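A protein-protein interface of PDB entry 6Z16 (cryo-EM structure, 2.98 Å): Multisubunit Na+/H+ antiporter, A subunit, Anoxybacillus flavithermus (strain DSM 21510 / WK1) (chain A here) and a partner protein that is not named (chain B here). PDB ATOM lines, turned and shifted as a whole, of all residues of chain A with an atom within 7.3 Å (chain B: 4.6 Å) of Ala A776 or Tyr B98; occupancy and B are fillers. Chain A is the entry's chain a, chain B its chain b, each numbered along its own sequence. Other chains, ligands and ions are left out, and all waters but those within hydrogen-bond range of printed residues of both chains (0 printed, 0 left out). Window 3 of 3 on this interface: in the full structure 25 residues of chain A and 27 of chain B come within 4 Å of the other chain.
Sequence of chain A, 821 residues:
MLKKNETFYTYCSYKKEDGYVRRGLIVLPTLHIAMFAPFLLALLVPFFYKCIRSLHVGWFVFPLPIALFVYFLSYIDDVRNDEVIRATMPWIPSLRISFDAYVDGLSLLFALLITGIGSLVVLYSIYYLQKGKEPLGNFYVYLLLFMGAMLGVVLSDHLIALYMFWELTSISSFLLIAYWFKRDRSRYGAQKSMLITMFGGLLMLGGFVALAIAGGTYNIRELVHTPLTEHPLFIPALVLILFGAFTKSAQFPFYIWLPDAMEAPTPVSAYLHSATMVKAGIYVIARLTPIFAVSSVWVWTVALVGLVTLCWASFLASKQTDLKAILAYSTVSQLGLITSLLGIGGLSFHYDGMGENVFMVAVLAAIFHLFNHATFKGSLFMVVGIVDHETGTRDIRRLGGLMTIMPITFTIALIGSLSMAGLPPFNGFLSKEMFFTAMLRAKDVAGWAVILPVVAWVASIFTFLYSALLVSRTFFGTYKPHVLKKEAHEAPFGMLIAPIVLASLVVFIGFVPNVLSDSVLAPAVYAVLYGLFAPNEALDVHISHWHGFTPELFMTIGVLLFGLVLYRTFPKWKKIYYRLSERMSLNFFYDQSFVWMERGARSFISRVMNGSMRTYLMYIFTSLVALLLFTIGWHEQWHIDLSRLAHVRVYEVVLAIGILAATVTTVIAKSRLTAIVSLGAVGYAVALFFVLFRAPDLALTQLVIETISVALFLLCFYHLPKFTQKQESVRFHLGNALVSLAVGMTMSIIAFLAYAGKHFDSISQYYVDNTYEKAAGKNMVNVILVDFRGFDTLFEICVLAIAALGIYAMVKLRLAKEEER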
ATOM      1  N   ASN A 770     -11.777 -15.277  16.795  1.00  0.00           N
ATOM      2  CA  ASN A 770     -11.772 -14.852  15.400  1.00  0.00           C
ATOM      3  C   ASN A 770     -13.169 -14.818  14.798  1.00  0.00           C
ATOM      4  O   ASN A 770     -13.344 -15.136  13.623  1.00  0.00           O
ATOM      5  CB  ASN A 770     -10.862 -15.752  14.568  1.00  0.00           C
ATOM      6  CG  ASN A 770      -9.398 -15.548  14.883  1.00  0.00           C
ATOM      7  OD1 ASN A 770      -8.935 -14.419  15.029  1.00  0.00           O
ATOM      8  ND2 ASN A 770      -8.662 -16.642  15.002  1.00  0.00           N
ATOM      9  N   THR A 771     -14.179 -14.437  15.578  1.00  0.00           N
ATOM     10  CA  THR A 771     -15.491 -14.201  14.988  1.00  0.00           C
ATOM     11  C   THR A 771     -15.582 -12.799  14.405  1.00  0.00           C
ATOM     12  O   THR A 771     -16.207 -12.601  13.359  1.00  0.00           O
ATOM     13  CB  THR A 771     -16.589 -14.445  16.027  1.00  0.00           C
ATOM     14  OG1 THR A 771     -16.484 -15.784  16.510  1.00  0.00           O
ATOM     15  CG2 THR A 771     -17.978 -14.286  15.438  1.00  0.00           C
ATOM     16  N   TYR A 772     -14.926 -11.825  15.028  1.00  0.00           N
ATOM     17  CA  TYR A 772     -14.927 -10.464  14.515  1.00  0.00           C
ATOM     18  C   TYR A 772     -13.629 -10.065  13.831  1.00  0.00           C
ATOM     19  O   TYR A 772     -13.668  -9.287  12.878  1.00  0.00           O
ATOM     20  CB  TYR A 772     -15.228  -9.474  15.647  1.00  0.00           C
ATOM     21  CG  TYR A 772     -15.266  -8.034  15.205  1.00  0.00           C
ATOM     22  CD1 TYR A 772     -16.328  -7.550  14.457  1.00  0.00           C
ATOM     23  CD2 TYR A 772     -14.236  -7.161  15.532  1.00  0.00           C
ATOM     24  CE1 TYR A 772     -16.364  -6.239  14.044  1.00  0.00           C
ATOM     25  CE2 TYR A 772     -14.263  -5.848  15.126  1.00  0.00           C
ATOM     26  CZ  TYR A 772     -15.329  -5.391  14.384  1.00  0.00           C
ATOM     27  OH  TYR A 772     -15.357  -4.078  13.978  1.00  0.00           O
ATOM     28  N   GLU A 773     -12.484 -10.580  14.279  1.00  0.00           N
ATOM     29  CA  GLU A 773     -11.216 -10.192  13.674  1.00  0.00           C
ATOM     30  C   GLU A 773     -11.023 -10.782  12.284  1.00  0.00           C
ATOM     31  O   GLU A 773     -10.273 -10.214  11.487  1.00  0.00           O
ATOM     32  CB  GLU A 773     -10.051 -10.610  14.570  1.00  0.00           C
ATOM     33  CG  GLU A 773      -9.991  -9.895  15.909  1.00  0.00           C
ATOM     34  CD  GLU A 773      -9.628  -8.426  15.785  1.00  0.00           C
ATOM     35  OE1 GLU A 773      -8.872  -8.072  14.856  1.00  0.00           O
ATOM     36  OE2 GLU A 773     -10.095  -7.627  16.624  1.00  0.00           O
ATOM     37  N   LYS A 774     -11.674 -11.899  11.976  1.00  0.00           N
ATOM     38  CA  LYS A 774     -11.558 -12.535  10.667  1.00  0.00           C
ATOM     39  C   LYS A 774     -12.867 -12.584   9.901  1.00  0.00           C
ATOM     40  O   LYS A 774     -12.890 -12.259   8.715  1.00  0.00           O
ATOM     41  CB  LYS A 774     -11.003 -13.955  10.814  1.00  0.00           C
ATOM     42  CG  LYS A 774      -9.588 -14.013  11.347  1.00  0.00           C
ATOM     43  CD  LYS A 774      -8.598 -13.490  10.325  1.00  0.00           C
ATOM     44  CE  LYS A 774      -7.184 -13.504  10.875  1.00  0.00           C
ATOM     45  NZ  LYS A 774      -6.693 -14.891  11.095  1.00  0.00           N
ATOM     46  N   ALA A 775     -13.958 -12.987  10.538  1.00  0.00           N
ATOM     47  CA  ALA A 775     -15.273 -12.889   9.934  1.00  0.00           C
ATOM     48  C   ALA A 775     -15.896 -11.548  10.312  1.00  0.00           C
ATOM     49  O   ALA A 775     -15.280 -10.709  10.970  1.00  0.00           O
ATOM     50  CB  ALA A 775     -16.156 -14.060  10.363  1.00  0.00           C
ATOM     51  N   ALA A 776     -17.127 -11.334   9.882  1.00  0.00           N
ATOM     52  CA  ALA A 776     -17.844 -10.097  10.172  1.00  0.00           C
ATOM     53  C   ALA A 776     -19.048 -10.460  11.033  1.00  0.00           C
ATOM     54  O   ALA A 776     -20.142 -10.713  10.523  1.00  0.00           O
ATOM     55  CB  ALA A 776     -18.263  -9.389   8.892  1.00  0.00           C
ATOM     56  N   GLY A 777     -18.841 -10.489  12.344  1.00  0.00           N
ATOM     57  CA  GLY A 777     -19.923 -10.845  13.235  1.00  0.00           C
ATOM     58  C   GLY A 777     -19.599 -10.697  14.703  1.00  0.00           C
ATOM     59  O   GLY A 777     -18.436 -10.770  15.110  1.00  0.00           O
ATOM     60  N   LYS A 778     -20.632 -10.467  15.504  1.00  0.00           N
ATOM     61  CA  LYS A 778     -20.530 -10.483  16.954  1.00  0.00           C
ATOM     62  C   LYS A 778     -21.253 -11.660  17.573  1.00  0.00           C
ATOM     63  O   LYS A 778     -20.797 -12.193  18.584  1.00  0.00           O
ATOM     64  CB  LYS A 778     -21.083  -9.185  17.544  1.00  0.00           C
ATOM     65  CG  LYS A 778     -20.320  -7.944  17.147  1.00  0.00           C
ATOM     66  CD  LYS A 778     -18.945  -7.917  17.757  1.00  0.00           C
ATOM     67  CE  LYS A 778     -18.236  -6.633  17.399  1.00  0.00           C
ATOM     68  NZ  LYS A 778     -18.901  -5.463  18.025  1.00  0.00           N
ATOM     69  N   ASN A 779     -22.380 -12.060  16.988  1.00  0.00           N
ATOM     70  CA  ASN A 779     -23.001 -13.329  17.327  1.00  0.00           C
ATOM     71  C   ASN A 779     -22.049 -14.449  16.950  1.00  0.00           C
ATOM     72  O   ASN A 779     -21.308 -14.344  15.976  1.00  0.00           O
ATOM     73  CB  ASN A 779     -24.318 -13.485  16.575  1.00  0.00           C
ATOM     74  CG  ASN A 779     -25.165 -14.612  17.100  1.00  0.00           C
ATOM     75  OD1 ASN A 779     -24.799 -15.291  18.052  1.00  0.00           O
ATOM     76  ND2 ASN A 779     -26.315 -14.816  16.482  1.00  0.00           N
ATOM     77  N   VAL A 783     -22.485 -17.181  13.157  1.00  0.00           N
ATOM     78  CA  VAL A 783     -21.266 -17.162  12.353  1.00  0.00           C
ATOM     79  C   VAL A 783     -20.715 -18.576  12.172  1.00  0.00           C
ATOM     80  O   VAL A 783     -20.219 -18.926  11.095  1.00  0.00           O
ATOM     81  CB  VAL A 783     -20.247 -16.192  12.980  1.00  0.00           C
ATOM     82  CG1 VAL A 783     -18.890 -16.291  12.333  1.00  0.00           C
ATOM     83  CG2 VAL A 783     -20.747 -14.782  12.807  1.00  0.00           C
ATOM     84  N   ASP A 787     -20.643 -19.291   8.356  1.00  0.00           N
ATOM     85  CA  ASP A 787     -19.323 -18.939   7.851  1.00  0.00           C
ATOM     86  C   ASP A 787     -18.281 -20.009   8.152  1.00  0.00           C
ATOM     87  O   ASP A 787     -17.636 -20.500   7.222  1.00  0.00           O
ATOM     88  CB  ASP A 787     -18.912 -17.578   8.421  1.00  0.00           C
ATOM     89  CG  ASP A 787     -17.700 -17.005   7.740  1.00  0.00           C
ATOM     90  OD1 ASP A 787     -17.827 -16.543   6.590  1.00  0.00           O
ATOM     91  OD2 ASP A 787     -16.623 -17.007   8.357  1.00  0.00           O
ATOM     92  N   HIS B  31     -26.036 -11.431  12.424  1.00  0.00           N
ATOM     93  CA  HIS B  31     -24.601 -11.540  12.653  1.00  0.00           C
ATOM     94  C   HIS B  31     -24.133 -10.893  13.944  1.00  0.00           C
ATOM     95  O   HIS B  31     -23.039 -11.220  14.415  1.00  0.00           O
ATOM     96  CB  HIS B  31     -23.807 -10.923  11.502  1.00  0.00           C
ATOM     97  CG  HIS B  31     -23.660 -11.818  10.317  1.00  0.00           C
ATOM     98  ND1 HIS B  31     -23.050 -11.409   9.152  1.00  0.00           N
ATOM     99  CD2 HIS B  31     -24.024 -13.106  10.119  1.00  0.00           C
ATOM    100  CE1 HIS B  31     -23.050 -12.403   8.286  1.00  0.00           C
ATOM    101  NE2 HIS B  31     -23.635 -13.445   8.847  1.00  0.00           N
ATOM    102  N   HIS B  96     -16.776 -16.461   1.102  1.00  0.00           N
ATOM    103  CA  HIS B  96     -17.529 -15.369   1.737  1.00  0.00           C
ATOM    104  C   HIS B  96     -16.664 -14.133   2.012  1.00  0.00           C
ATOM    105  O   HIS B  96     -16.343 -13.800   3.151  1.00  0.00           O
ATOM    106  CB  HIS B  96     -18.224 -15.842   3.020  1.00  0.00           C
ATOM    107  CG  HIS B  96     -19.437 -16.678   2.774  1.00  0.00           C
ATOM    108  ND1 HIS B  96     -20.056 -17.403   3.766  1.00  0.00           N
ATOM    109  CD2 HIS B  96     -20.160 -16.885   1.650  1.00  0.00           C
ATOM    110  CE1 HIS B  96     -21.102 -18.031   3.262  1.00  0.00           C
ATOM    111  NE2 HIS B  96     -21.188 -17.732   1.980  1.00  0.00           N
ATOM    112  N   ALA B  97     -16.279 -13.470   0.925  1.00  0.00           N
ATOM    113  CA  ALA B  97     -15.717 -12.128   1.007  1.00  0.00           C
ATOM    114  C   ALA B  97     -16.834 -11.094   0.838  1.00  0.00           C
ATOM    115  O   ALA B  97     -18.019 -11.434   0.794  1.00  0.00           O
ATOM    116  CB  ALA B  97     -14.613 -11.952  -0.031  1.00  0.00           C
ATOM    117  N   TYR B  98     -16.474  -9.815   0.742  1.00  0.00           N
ATOM    118  CA  TYR B  98     -17.467  -8.753   0.636  1.00  0.00           C
ATOM    119  C   TYR B  98     -17.942  -8.590  -0.803  1.00  0.00           C
ATOM    120  O   TYR B  98     -17.351  -9.115  -1.747  1.00  0.00           O
ATOM    121  CB  TYR B  98     -16.907  -7.429   1.143  1.00  0.00           C
ATOM    122  CG  TYR B  98     -16.668  -7.395   2.628  1.00  0.00           C
ATOM    123  CD1 TYR B  98     -17.715  -7.174   3.514  1.00  0.00           C
ATOM    124  CD2 TYR B  98     -15.395  -7.584   3.144  1.00  0.00           C
ATOM    125  CE1 TYR B  98     -17.498  -7.142   4.876  1.00  0.00           C
ATOM    126  CE2 TYR B  98     -15.166  -7.555   4.505  1.00  0.00           C
ATOM    127  CZ  TYR B  98     -16.221  -7.335   5.364  1.00  0.00           C
ATOM    128  OH  TYR B  98     -15.989  -7.305   6.718  1.00  0.00           O
ATOM    129  N   LYS B  99     -19.027  -7.834  -0.965  1.00  0.00           N
ATOM    130  CA  LYS B  99     -19.626  -7.650  -2.280  1.00  0.00           C
ATOM    131  C   LYS B  99     -20.379  -6.331  -2.322  1.00  0.00           C
ATOM    132  O   LYS B  99     -21.135  -6.013  -1.398  1.00  0.00           O
ATOM    133  CB  LYS B  99     -20.570  -8.805  -2.618  1.00  0.00           C
ATOM    134  CG  LYS B  99     -21.139  -8.784  -4.023  1.00  0.00           C
ATOM    135  CD  LYS B  99     -21.985 -10.022  -4.278  1.00  0.00           C
ATOM    136  CE  LYS B  99     -22.452 -10.103  -5.722  1.00  0.00           C
ATOM    137  NZ  LYS B  99     -23.429  -9.033  -6.063  1.00  0.00           N
ATOM    138  N   TYR B 100     -20.164  -5.574  -3.393  1.00  0.00           N
ATOM    139  CA  TYR B 100     -20.869  -4.322  -3.634  1.00  0.00           C
ATOM    140  C   TYR B 100     -22.102  -4.592  -4.482  1.00  0.00           C
ATOM    141  O   TYR B 100     -22.028  -5.318  -5.476  1.00  0.00           O
ATOM    142  CB  TYR B 100     -19.962  -3.324  -4.354  1.00  0.00           C
ATOM    143  CG  TYR B 100     -18.788  -2.831  -3.546  1.00  0.00           C
ATOM    144  CD1 TYR B 100     -18.917  -1.749  -2.687  1.00  0.00           C
ATOM    145  CD2 TYR B 100     -17.549  -3.452  -3.641  1.00  0.00           C
ATOM    146  CE1 TYR B 100     -17.842  -1.293  -1.950  1.00  0.00           C
ATOM    147  CE2 TYR B 100     -16.471  -3.007  -2.906  1.00  0.00           C
ATOM    148  CZ  TYR B 100     -16.623  -1.929  -2.062  1.00  0.00           C
ATOM    149  OH  TYR B 100     -15.548  -1.482  -1.329  1.00  0.00           O
ATOM    150  N   LEU B 111     -21.763  -5.300   1.374  1.00  0.00           N
ATOM    151  CA  LEU B 111     -22.268  -6.238   2.360  1.00  0.00           C
ATOM    152  C   LEU B 111     -21.416  -7.500   2.384  1.00  0.00           C
ATOM    153  O   LEU B 111     -20.655  -7.790   1.456  1.00  0.00           O
ATOM    154  CB  LEU B 111     -23.746  -6.572   2.094  1.00  0.00           C
ATOM    155  CG  LEU B 111     -24.202  -7.116   0.738  1.00  0.00           C
ATOM    156  CD1 LEU B 111     -24.164  -8.636   0.654  1.00  0.00           C
ATOM    157  CD2 LEU B 111     -25.592  -6.597   0.409  1.00  0.00           C
ATOM    158  N   HIS B 112     -21.557  -8.247   3.471  1.00  0.00           N
ATOM    159  CA  HIS B 112     -20.902  -9.534   3.608  1.00  0.00           C
ATOM    160  C   HIS B 112     -21.821 -10.606   3.038  1.00  0.00           C
ATOM    161  O   HIS B 112     -23.024 -10.612   3.309  1.00  0.00           O
ATOM    162  CB  HIS B 112     -20.595  -9.798   5.080  1.00  0.00           C
ATOM    163  CG  HIS B 112     -19.592 -10.879   5.316  1.00  0.00           C
ATOM    164  ND1 HIS B 112     -19.933 -12.211   5.394  1.00  0.00           N
ATOM    165  CD2 HIS B 112     -18.256 -10.822   5.521  1.00  0.00           C
ATOM    166  CE1 HIS B 112     -18.848 -12.928   5.622  1.00  0.00           C
ATOM    167  NE2 HIS B 112     -17.817 -12.109   5.702  1.00  0.00           N
ATOM    168  N   THR B 113     -21.261 -11.508   2.235  1.00  0.00           N
ATOM    169  CA  THR B 113     -22.086 -12.434   1.463  1.00  0.00           C
ATOM    170  C   THR B 113     -22.648 -13.590   2.278  1.00  0.00           C
ATOM    171  O   THR B 113     -23.379 -14.413   1.720  1.00  0.00           O
ATOM    172  CB  THR B 113     -21.300 -12.993   0.281  1.00  0.00           C
ATOM    173  OG1 THR B 113     -20.111 -13.624   0.756  1.00  0.00           O
ATOM    174  CG2 THR B 113     -20.934 -11.899  -0.678  1.00  0.00           C
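The backbone NH (N) of Lys A778 sits at hydrogen-bond distance from the backbone carbonyl oxygen (O) of His B31, 2.7 Å away.
A ring nitrogen (ND1) of His B31 sits at hydrogen-bond distance from the backbone carbonyl oxygen of Ala A776.
N of Asn A779 is in hydrogen-bond range of O of His B31.
Thr A771 touches none of the printed residues of chain B.
Ala A776 touches just these residues of chain B: His B31, Tyr B98 and His B112.
Of the printed residues of chain B, Gly A777 touches His B31.
Of the printed residues of chain B, Asn A779 touches His B31.
Printed residues of chain A within 4 Å of His B31: Ala A776 (3.3 Å), Gly A777 (3.4 Å), Lys A778 (2.7 Å) and Asn A779 (2.8 Å).
Tyr B98 touches just one residue of chain A: Ala A776.
Of the printed residues of chain A, His B112 touches Ala A776 (3.7 Å) and Asp A787 (3.9 Å).
Thr B113 touches none of the printed residues of chain A.
The nearest printed residue of chain A that does not touch His B112 is Ala A775 (5.0 Å).
The backbone carbonyl oxygen (O) of His B96 sits at hydrogen-bond distance from a ring nitrogen (NE2) of His B112 (3.4 Å).
Of the 12 printed residues of chain A, 5 touch a printed residue of chain B.
Hydrophobic or aromatic side chains of chain B that line the printed part of chain A: His B31, His B96, Tyr B98 and His B112.
Among the printed residues, 8 pairs touch across the chains.
Among the printed residues, no Asp or Glu carboxylate lies within 4 Å of a Lys or Arg side-chain nitrogen of the other chain.
OH of Tyr B98 touches CB of Ala A776 (3.8 Å).
His B112 touches Ala A776 (CD2 to CB, 3.7 Å).
Gly A777 touches His B31 (CA to O, 3.4 Å).
CB of His B96 touches OD1 of Asp A787, at 3.7 Å.
Asp A787 touches His B112.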
